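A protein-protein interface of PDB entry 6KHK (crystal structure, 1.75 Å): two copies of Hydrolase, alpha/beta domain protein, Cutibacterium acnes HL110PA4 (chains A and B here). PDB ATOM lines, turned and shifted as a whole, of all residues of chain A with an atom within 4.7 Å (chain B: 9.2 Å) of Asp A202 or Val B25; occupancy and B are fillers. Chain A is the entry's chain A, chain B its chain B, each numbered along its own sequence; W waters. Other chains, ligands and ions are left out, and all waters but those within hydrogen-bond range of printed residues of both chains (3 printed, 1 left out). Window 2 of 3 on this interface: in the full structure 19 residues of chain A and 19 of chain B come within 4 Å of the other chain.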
ATOM      1  N   GLU A 198     -17.653  12.536  17.146  1.00  0.00           N
ATOM      2  CA  GLU A 198     -17.172  13.194  15.902  1.00  0.00           C
ATOM      3  C   GLU A 198     -17.898  12.571  14.704  1.00  0.00           C
ATOM      4  O   GLU A 198     -18.496  13.330  13.916  1.00  0.00           O
ATOM      5  CB  GLU A 198     -15.657  13.030  15.764  1.00  0.00           C
ATOM      6  CG  GLU A 198     -14.862  13.983  16.638  1.00  0.00           C
ATOM      7  CD  GLU A 198     -13.354  13.857  16.500  1.00  0.00           C
ATOM      8  OE1 GLU A 198     -12.905  13.066  15.647  1.00  0.00           O
ATOM      9  OE2 GLU A 198     -12.634  14.548  17.247  1.00  0.00           O
ATOM     10  N   VAL A 199     -17.841  11.241  14.584  1.00  0.00           N
ATOM     11  CA  VAL A 199     -18.520  10.526  13.468  1.00  0.00           C
ATOM     12  C   VAL A 199     -20.000  10.932  13.445  1.00  0.00           C
ATOM     13  O   VAL A 199     -20.469  11.209  12.409  1.00  0.00           O
ATOM     14  CB  VAL A 199     -18.363   8.994  13.519  1.00  0.00           C
ATOM     15  CG1 VAL A 199     -19.260   8.293  12.514  1.00  0.00           C
ATOM     16  CG2 VAL A 199     -16.935   8.572  13.308  1.00  0.00           C
ATOM     17  N   VAL A 200     -20.680  10.971  14.588  1.00  0.00           N
ATOM     18  CA  VAL A 200     -22.142  11.292  14.588  1.00  0.00           C
ATOM     19  C   VAL A 200     -22.324  12.726  14.078  1.00  0.00           C
ATOM     20  O   VAL A 200     -23.245  12.982  13.251  1.00  0.00           O
ATOM     21  CB  VAL A 200     -22.780  11.128  15.990  1.00  0.00           C
ATOM     22  CG1 VAL A 200     -24.277  11.440  15.930  1.00  0.00           C
ATOM     23  CG2 VAL A 200     -22.494   9.736  16.532  1.00  0.00           C
ATOM     24  N   ALA A 201     -21.446  13.644  14.488  1.00  0.00           N
ATOM     25  CA  ALA A 201     -21.581  15.063  14.101  1.00  0.00           C
ATOM     26  C   ALA A 201     -21.389  15.160  12.588  1.00  0.00           C
ATOM     27  O   ALA A 201     -22.097  15.938  11.987  1.00  0.00           O
ATOM     28  CB  ALA A 201     -20.571  15.927  14.839  1.00  0.00           C
ATOM     29  N   ASP A 202     -20.406  14.439  12.024  1.00  0.00           N
ATOM     30  CA  ASP A 202     -20.133  14.482  10.557  1.00  0.00           C
ATOM     31  C   ASP A 202     -21.346  13.874   9.812  1.00  0.00           C
ATOM     32  O   ASP A 202     -21.848  14.434   8.776  1.00  0.00           O
ATOM     33  CB  ASP A 202     -18.821  13.792  10.229  1.00  0.00           C
ATOM     34  CG  ASP A 202     -18.633  13.728   8.738  1.00  0.00           C
ATOM     35  OD1 ASP A 202     -18.231  14.780   8.160  1.00  0.00           O
ATOM     36  OD2 ASP A 202     -19.020  12.690   8.162  1.00  0.00           O
ATOM     37  N   HIS A 203     -21.886  12.777  10.335  1.00  0.00           N
ATOM     38  CA  HIS A 203     -23.098  12.131   9.785  1.00  0.00           C
ATOM     39  C   HIS A 203     -24.233  13.157   9.711  1.00  0.00           C
ATOM     40  O   HIS A 203     -24.941  13.210   8.690  1.00  0.00           O
ATOM     41  CB  HIS A 203     -23.457  10.916  10.628  1.00  0.00           C
ATOM     42  CG  HIS A 203     -24.758  10.279  10.289  1.00  0.00           C
ATOM     43  ND1 HIS A 203     -25.925  10.604  10.964  1.00  0.00           N
ATOM     44  CD2 HIS A 203     -25.080   9.294   9.424  1.00  0.00           C
ATOM     45  CE1 HIS A 203     -26.922   9.872  10.484  1.00  0.00           C
ATOM     46  NE2 HIS A 203     -26.420   9.019   9.589  1.00  0.00           N
ATOM     47  N   GLY A 204     -24.409  13.979  10.748  1.00  0.00           N
ATOM     48  CA  GLY A 204     -25.466  14.994  10.771  1.00  0.00           C
ATOM     49  C   GLY A 204     -25.263  16.119   9.776  1.00  0.00           C
ATOM     50  O   GLY A 204     -26.270  16.660   9.279  1.00  0.00           O
ATOM     51  N   LYS A 205     -24.013  16.486   9.535  1.00  0.00           N
ATOM     52  CA  LYS A 205     -23.636  17.687   8.751  1.00  0.00           C
ATOM     53  C   LYS A 205     -23.629  17.376   7.254  1.00  0.00           C
ATOM     54  O   LYS A 205     -24.008  18.259   6.459  1.00  0.00           O
ATOM     55  CB  LYS A 205     -22.256  18.181   9.207  1.00  0.00           C
ATOM     56  CG  LYS A 205     -21.896  19.574   8.706  1.00  0.00           C
ATOM     57  CD  LYS A 205     -20.486  20.007   9.053  1.00  0.00           C
ATOM     58  CE  LYS A 205     -19.550  19.778   7.884  1.00  0.00           C
ATOM     59  NZ  LYS A 205     -18.186  19.405   8.324  1.00  0.00           N
ATOM     60  N   ASP A 206     -23.305  16.141   6.865  1.00  0.00           N
ATOM     61  CA  ASP A 206     -23.076  15.755   5.443  1.00  0.00           C
ATOM     62  C   ASP A 206     -24.343  15.956   4.625  1.00  0.00           C
ATOM     63  O   ASP A 206     -25.354  15.257   4.860  1.00  0.00           O
ATOM     64  CB  ASP A 206     -22.649  14.292   5.364  1.00  0.00           C
ATOM     65  CG  ASP A 206     -22.048  13.811   4.052  1.00  0.00           C
ATOM     66  OD1 ASP A 206     -22.288  14.425   2.987  1.00  0.00           O
ATOM     67  OD2 ASP A 206     -21.463  12.736   4.093  1.00  0.00           O
ATOM     68  N   ASN A 209     -26.114  12.886   3.129  1.00  0.00           N
ATOM     69  CA  ASN A 209     -26.926  12.021   4.024  1.00  0.00           C
ATOM     70  C   ASN A 209     -28.328  12.574   4.086  1.00  0.00           C
ATOM     71  O   ASN A 209     -29.289  11.873   3.721  1.00  0.00           O
ATOM     72  CB  ASN A 209     -26.346  11.980   5.436  1.00  0.00           C
ATOM     73  CG  ASN A 209     -25.061  11.190   5.534  1.00  0.00           C
ATOM     74  OD1 ASN A 209     -24.698  10.405   4.630  1.00  0.00           O
ATOM     75  ND2 ASN A 209     -24.318  11.382   6.621  1.00  0.00           N
ATOM     76  N   ALA B   2     -17.748  14.569   5.441  1.00  0.00           N
ATOM     77  CA  ALA B   2     -18.815  15.208   4.664  1.00  0.00           C
ATOM     78  C   ALA B   2     -18.279  15.498   3.258  1.00  0.00           C
ATOM     79  O   ALA B   2     -17.038  15.684   3.104  1.00  0.00           O
ATOM     80  CB  ALA B   2     -19.245  16.480   5.311  1.00  0.00           C
ATOM     81  N   LEU B   3     -19.200  15.593   2.314  1.00  0.00           N
ATOM     82  CA  LEU B   3     -18.898  15.836   0.893  1.00  0.00           C
ATOM     83  C   LEU B   3     -19.726  17.022   0.444  1.00  0.00           C
ATOM     84  O   LEU B   3     -20.956  17.042   0.704  1.00  0.00           O
ATOM     85  CB  LEU B   3     -19.231  14.612   0.052  1.00  0.00           C
ATOM     86  CG  LEU B   3     -19.021  14.778  -1.460  1.00  0.00           C
ATOM     87  CD1 LEU B   3     -17.533  14.989  -1.758  1.00  0.00           C
ATOM     88  CD2 LEU B   3     -19.546  13.562  -2.229  1.00  0.00           C
ATOM     89  N   GLN B   4     -19.063  17.973  -0.209  1.00  0.00           N
ATOM     90  CA  GLN B   4     -19.755  19.091  -0.879  1.00  0.00           C
ATOM     91  C   GLN B   4     -19.488  18.989  -2.374  1.00  0.00           C
ATOM     92  O   GLN B   4     -18.331  18.778  -2.749  1.00  0.00           O
ATOM     93  CB  GLN B   4     -19.278  20.449  -0.348  1.00  0.00           C
ATOM     94  CG  GLN B   4     -19.539  20.716   1.123  1.00  0.00           C
ATOM     95  CD  GLN B   4     -19.155  22.141   1.452  1.00  0.00           C
ATOM     96  OE1 GLN B   4     -19.618  23.084   0.810  1.00  0.00           O
ATOM     97  NE2 GLN B   4     -18.239  22.293   2.380  1.00  0.00           N
ATOM     98  N   ALA B  21     -15.516  19.476  -2.298  1.00  0.00           N
ATOM     99  CA  ALA B  21     -14.794  19.657  -1.031  1.00  0.00           C
ATOM    100  C   ALA B  21     -15.047  18.414  -0.199  1.00  0.00           C
ATOM    101  O   ALA B  21     -16.230  17.966  -0.101  1.00  0.00           O
ATOM    102  CB  ALA B  21     -15.222  20.910  -0.285  1.00  0.00           C
ATOM    103  N   TYR B  22     -13.992  17.929   0.401  1.00  0.00           N
ATOM    104  CA  TYR B  22     -13.960  16.742   1.296  1.00  0.00           C
ATOM    105  C   TYR B  22     -13.579  17.173   2.716  1.00  0.00           C
ATOM    106  O   TYR B  22     -12.471  17.749   2.933  1.00  0.00           O
ATOM    107  CB  TYR B  22     -12.982  15.724   0.728  1.00  0.00           C
ATOM    108  CG  TYR B  22     -13.111  15.402  -0.736  1.00  0.00           C
ATOM    109  CD1 TYR B  22     -13.908  14.351  -1.179  1.00  0.00           C
ATOM    110  CD2 TYR B  22     -12.429  16.134  -1.698  1.00  0.00           C
ATOM    111  CE1 TYR B  22     -13.967  13.982  -2.513  1.00  0.00           C
ATOM    112  CE2 TYR B  22     -12.461  15.766  -3.031  1.00  0.00           C
ATOM    113  CZ  TYR B  22     -13.282  14.726  -3.462  1.00  0.00           C
ATOM    114  OH  TYR B  22     -13.337  14.377  -4.778  1.00  0.00           O
ATOM    115  N   GLU B  23     -14.481  16.968   3.698  1.00  0.00           N
ATOM    116  CA  GLU B  23     -14.203  17.374   5.091  1.00  0.00           C
ATOM    117  C   GLU B  23     -13.991  16.141   5.950  1.00  0.00           C
ATOM    118  O   GLU B  23     -14.753  15.185   5.877  1.00  0.00           O
ATOM    119  CB  GLU B  23     -15.325  18.208   5.655  1.00  0.00           C
ATOM    120  CG  GLU B  23     -15.694  19.365   4.769  1.00  0.00           C
ATOM    121  CD  GLU B  23     -16.939  20.057   5.275  1.00  0.00           C
ATOM    122  OE1 GLU B  23     -17.902  20.173   4.522  1.00  0.00           O
ATOM    123  OE2 GLU B  23     -16.960  20.408   6.453  1.00  0.00           O
ATOM    124  N   PRO B  24     -12.929  16.129   6.762  1.00  0.00           N
ATOM    125  CA  PRO B  24     -12.683  15.018   7.657  1.00  0.00           C
ATOM    126  C   PRO B  24     -13.672  15.110   8.824  1.00  0.00           C
ATOM    127  O   PRO B  24     -14.312  16.132   9.069  1.00  0.00           O
ATOM    128  CB  PRO B  24     -11.231  15.242   8.087  1.00  0.00           C
ATOM    129  CG  PRO B  24     -11.072  16.715   8.056  1.00  0.00           C
ATOM    130  CD  PRO B  24     -12.049  17.269   7.044  1.00  0.00           C
ATOM    131  N   VAL B  25     -13.794  13.995   9.499  1.00  0.00           N
ATOM    132  CA  VAL B  25     -14.460  13.905  10.822  1.00  0.00           C
ATOM    133  C   VAL B  25     -13.660  14.764  11.806  1.00  0.00           C
ATOM    134  O   VAL B  25     -12.403  14.752  11.727  1.00  0.00           O
ATOM    135  CB  VAL B  25     -14.510  12.401  11.157  1.00  0.00           C
ATOM    136  CG1 VAL B  25     -14.408  12.114  12.633  1.00  0.00           C
ATOM    137  CG2 VAL B  25     -15.731  11.758  10.514  1.00  0.00           C
ATOM    138  N   GLY B  26     -14.330  15.445  12.730  1.00  0.00           N
ATOM    139  CA  GLY B  26     -13.630  16.217  13.762  1.00  0.00           C
ATOM    140  C   GLY B  26     -13.299  17.616  13.294  1.00  0.00           C
ATOM    141  O   GLY B  26     -14.022  18.162  12.437  1.00  0.00           O
ATOM    142  N   THR B  27     -12.274  18.206  13.887  1.00  0.00           N
ATOM    143  CA  THR B  27     -11.924  19.632  13.677  1.00  0.00           C
ATOM    144  C   THR B  27     -10.693  19.664  12.792  1.00  0.00           C
ATOM    145  O   THR B  27      -9.609  19.261  13.207  1.00  0.00           O
ATOM    146  CB  THR B  27     -11.685  20.374  14.991  1.00  0.00           C
ATOM    147  OG1 THR B  27     -12.896  20.214  15.734  1.00  0.00           O
ATOM    148  CG2 THR B  27     -11.373  21.837  14.777  1.00  0.00           C
ATOM    149  N   PRO B  28     -10.827  20.114  11.538  1.00  0.00           N
ATOM    150  CA  PRO B  28      -9.694  20.103  10.630  1.00  0.00           C
ATOM    151  C   PRO B  28      -8.701  21.185  11.055  1.00  0.00           C
ATOM    152  O   PRO B  28      -9.145  22.208  11.655  1.00  0.00           O
ATOM    153  CB  PRO B  28     -10.341  20.423   9.262  1.00  0.00           C
ATOM    154  CG  PRO B  28     -11.535  21.243   9.620  1.00  0.00           C
ATOM    155  CD  PRO B  28     -12.045  20.653  10.924  1.00  0.00           C
ATOM    156  N   THR B  29      -7.447  21.011  10.648  1.00  0.00           N
ATOM    157  CA  THR B  29      -6.324  21.902  11.030  1.00  0.00           C
ATOM    158  C   THR B  29      -5.748  22.647   9.821  1.00  0.00           C
ATOM    159  O   THR B  29      -4.785  23.414  10.003  1.00  0.00           O
ATOM    160  CB  THR B  29      -5.236  21.116  11.755  1.00  0.00           C
ATOM    161  OG1 THR B  29      -4.729  20.079  10.909  1.00  0.00           O
ATOM    162  CG2 THR B  29      -5.770  20.483  13.029  1.00  0.00           C
ATOM    163  N   LEU B  52      -4.977  12.694   3.192  1.00  0.00           N
ATOM    164  CA  LEU B  52      -5.037  14.080   3.734  1.00  0.00           C
ATOM    165  C   LEU B  52      -6.200  14.159   4.696  1.00  0.00           C
ATOM    166  O   LEU B  52      -6.010  14.814   5.730  1.00  0.00           O
ATOM    167  CB  LEU B  52      -5.149  15.107   2.605  1.00  0.00           C
ATOM    168  CG  LEU B  52      -3.962  15.163   1.657  1.00  0.00           C
ATOM    169  CD1 LEU B  52      -4.193  16.155   0.533  1.00  0.00           C
ATOM    170  CD2 LEU B  52      -2.692  15.561   2.427  1.00  0.00           C
ATOM    171  N   LEU B  53      -7.368  13.578   4.364  1.00  0.00           N
ATOM    172  CA  LEU B  53      -8.503  13.498   5.313  1.00  0.00           C
ATOM    173  C   LEU B  53      -8.041  12.775   6.580  1.00  0.00           C
ATOM    174  O   LEU B  53      -8.440  13.197   7.681  1.00  0.00           O
ATOM    175  CB  LEU B  53      -9.704  12.789   4.682  1.00  0.00           C
ATOM    176  CG  LEU B  53     -10.417  13.563   3.563  1.00  0.00           C
ATOM    177  CD1 LEU B  53     -11.397  12.655   2.852  1.00  0.00           C
ATOM    178  CD2 LEU B  53     -11.131  14.801   4.035  1.00  0.00           C
ATOM    179  N   ASP B  54      -7.354  11.651   6.436  1.00  0.00           N
ATOM    180  CA  ASP B  54      -6.832  10.853   7.559  1.00  0.00           C
ATOM    181  C   ASP B  54      -5.964  11.764   8.456  1.00  0.00           C
ATOM    182  O   ASP B  54      -6.012  11.616   9.687  1.00  0.00           O
ATOM    183  CB  ASP B  54      -6.042   9.636   7.067  1.00  0.00           C
ATOM    184  CG  ASP B  54      -6.905   8.548   6.473  1.00  0.00           C
ATOM    185  OD1 ASP B  54      -8.154   8.629   6.627  1.00  0.00           O
ATOM    186  OD2 ASP B  54      -6.349   7.682   5.786  1.00  0.00           O
ATOM    187  N   ALA B  55      -5.235  12.708   7.875  1.00  0.00           N
ATOM    188  CA  ALA B  55      -4.362  13.645   8.620  1.00  0.00           C
ATOM    189  C   ALA B  55      -5.138  14.811   9.241  1.00  0.00           C
ATOM    190  O   ALA B  55      -4.473  15.676   9.848  1.00  0.00           O
ATOM    191  CB  ALA B  55      -3.279  14.137   7.697  1.00  0.00           C
ATOM    192  N   GLY B  56      -6.453  14.942   9.037  1.00  0.00           N
ATOM    193  CA  GLY B  56      -7.247  16.041   9.650  1.00  0.00           C
ATOM    194  C   GLY B  56      -7.341  17.298   8.787  1.00  0.00           C
ATOM    195  O   GLY B  56      -7.577  18.397   9.337  1.00  0.00           O
ATOM    196  N   PHE B  57      -7.162  17.166   7.474  1.00  0.00           N
ATOM    197  CA  PHE B  57      -7.241  18.316   6.532  1.00  0.00           C
ATOM    198  C   PHE B  57      -8.526  18.257   5.704  1.00  0.00           C
ATOM    199  O   PHE B  57      -8.925  17.166   5.262  1.00  0.00           O
ATOM    200  CB  PHE B  57      -6.037  18.348   5.581  1.00  0.00           C
ATOM    201  CG  PHE B  57      -4.684  18.168   6.225  1.00  0.00           C
ATOM    202  CD1 PHE B  57      -4.427  18.679   7.481  1.00  0.00           C
ATOM    203  CD2 PHE B  57      -3.639  17.549   5.549  1.00  0.00           C
ATOM    204  CE1 PHE B  57      -3.176  18.537   8.085  1.00  0.00           C
ATOM    205  CE2 PHE B  57      -2.410  17.367   6.171  1.00  0.00           C
ATOM    206  CZ  PHE B  57      -2.197  17.850   7.438  1.00  0.00           C
ATOM    207  N   VAL B  58      -9.076  19.442   5.416  1.00  0.00           N
ATOM    208  CA  VAL B  58     -10.081  19.691   4.350  1.00  0.00           C
ATOM    209  C   VAL B  58      -9.324  19.621   3.011  1.00  0.00           C
ATOM    210  O   VAL B  58      -8.140  20.051   2.986  1.00  0.00           O
ATOM    211  CB  VAL B  58     -10.809  21.036   4.504  1.00  0.00           C
ATOM    212  CG1 VAL B  58     -11.715  21.286   3.304  1.00  0.00           C
ATOM    213  CG2 VAL B  58     -11.614  21.086   5.801  1.00  0.00           C
HETATM  214  O   HOH W   1     -17.490  17.007   8.835  1.00  0.00           O
HETATM  215  O   HOH W   2     -17.331  15.792  13.190  1.00  0.00           O
HETATM  216  O   HOH W   3     -10.650  16.406  15.843  1.00  0.00           O
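Glu A198 touches Val B25 (CB to CG1, 3.5 Å).
Glu A198 touches Gly B26 (CD to CA, 3.6 Å).
Asp A202 touches Val B25.
Asp A206 touches Ala B2.
Water W1 lies within hydrogen-bond range of OD1 of Asp A202 (2.4 Å), NZ of Lys A205 (2.5 Å) and O of Pro B24 (3.3 Å).
Water W2 lies within hydrogen-bond range of the backbone carbonyl oxygen (O) of Glu A198 (2.8 Å) and the backbone NH (N) of Gly B26 (3.1 Å).
Water W3 lies within hydrogen-bond range of OE2 of Glu A198 (3.1 Å) and N of Thr B27 (3.1 Å).
Asp A202 touches just these residues of chain B: Ala B2 (2.8 Å) and Val B25 (3.7 Å).
Val B25 touches just these residues of chain A: Glu A198 (3.5 Å) and Asp A202 (3.7 Å).
No residue of chain B comes within 4 Å of Ala A201.
No residue of chain B comes within 4 Å of Gly A204.
Printed residues of chain A within 4 Å of Glu B23: Lys A205 (2.5 Å).
Of the printed residues of chain A, Leu B3 touches Asp A206 (3.4 Å).
Of the printed residues of chain A, Ala B2 touches Asp A202 and Asp A206.
Printed residues of chain B within 4 Å of Glu A198: Val B25 and Gly B26.
Printed residues of chain B within 4 Å of Asp A206: Ala B2 (3.6 Å) and Leu B3 (3.4 Å).
Val A200 touches none of the printed residues of chain B.
No position is printed for both chains.
Of the 7 pairs that touch across the chains among the printed residues, none has its exchanged pair printed and touching as well.
The backbone NH (N) of Glu B23 sits at hydrogen-bond distance from the backbone carbonyl oxygen (O) of Ala B2 (2.9 Å).
NE2 of Gln B4 sits at hydrogen-bond distance from OE1 of Glu B23 (3.0 Å).
The side-chain carboxylate (OD1) of Asp A202 is in hydrogen-bond range of the backbone NH (N) of Ala B2.
The side-chain carboxylate (OE2) of Glu B23 lies within salt-bridge range of the side-chain amino group (NZ) of Lys A205 (2.5 Å).
The backbone NH of Leu B3 lies within hydrogen-bond range of the side-chain carboxylate of Asp A206 (3.4 Å).
Hydrophobic or aromatic side chains of chain B within 4 Å of the printed part of chain A: Ala B2 and Val B25.
Among the printed residues, 7 pairs touch across the chains.
Among the printed residues, Asp or Glu carboxylates within 4 Å of a Lys or Arg side-chain nitrogen of the other chain: Lys A205 with Glu B23 (2.5 Å).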
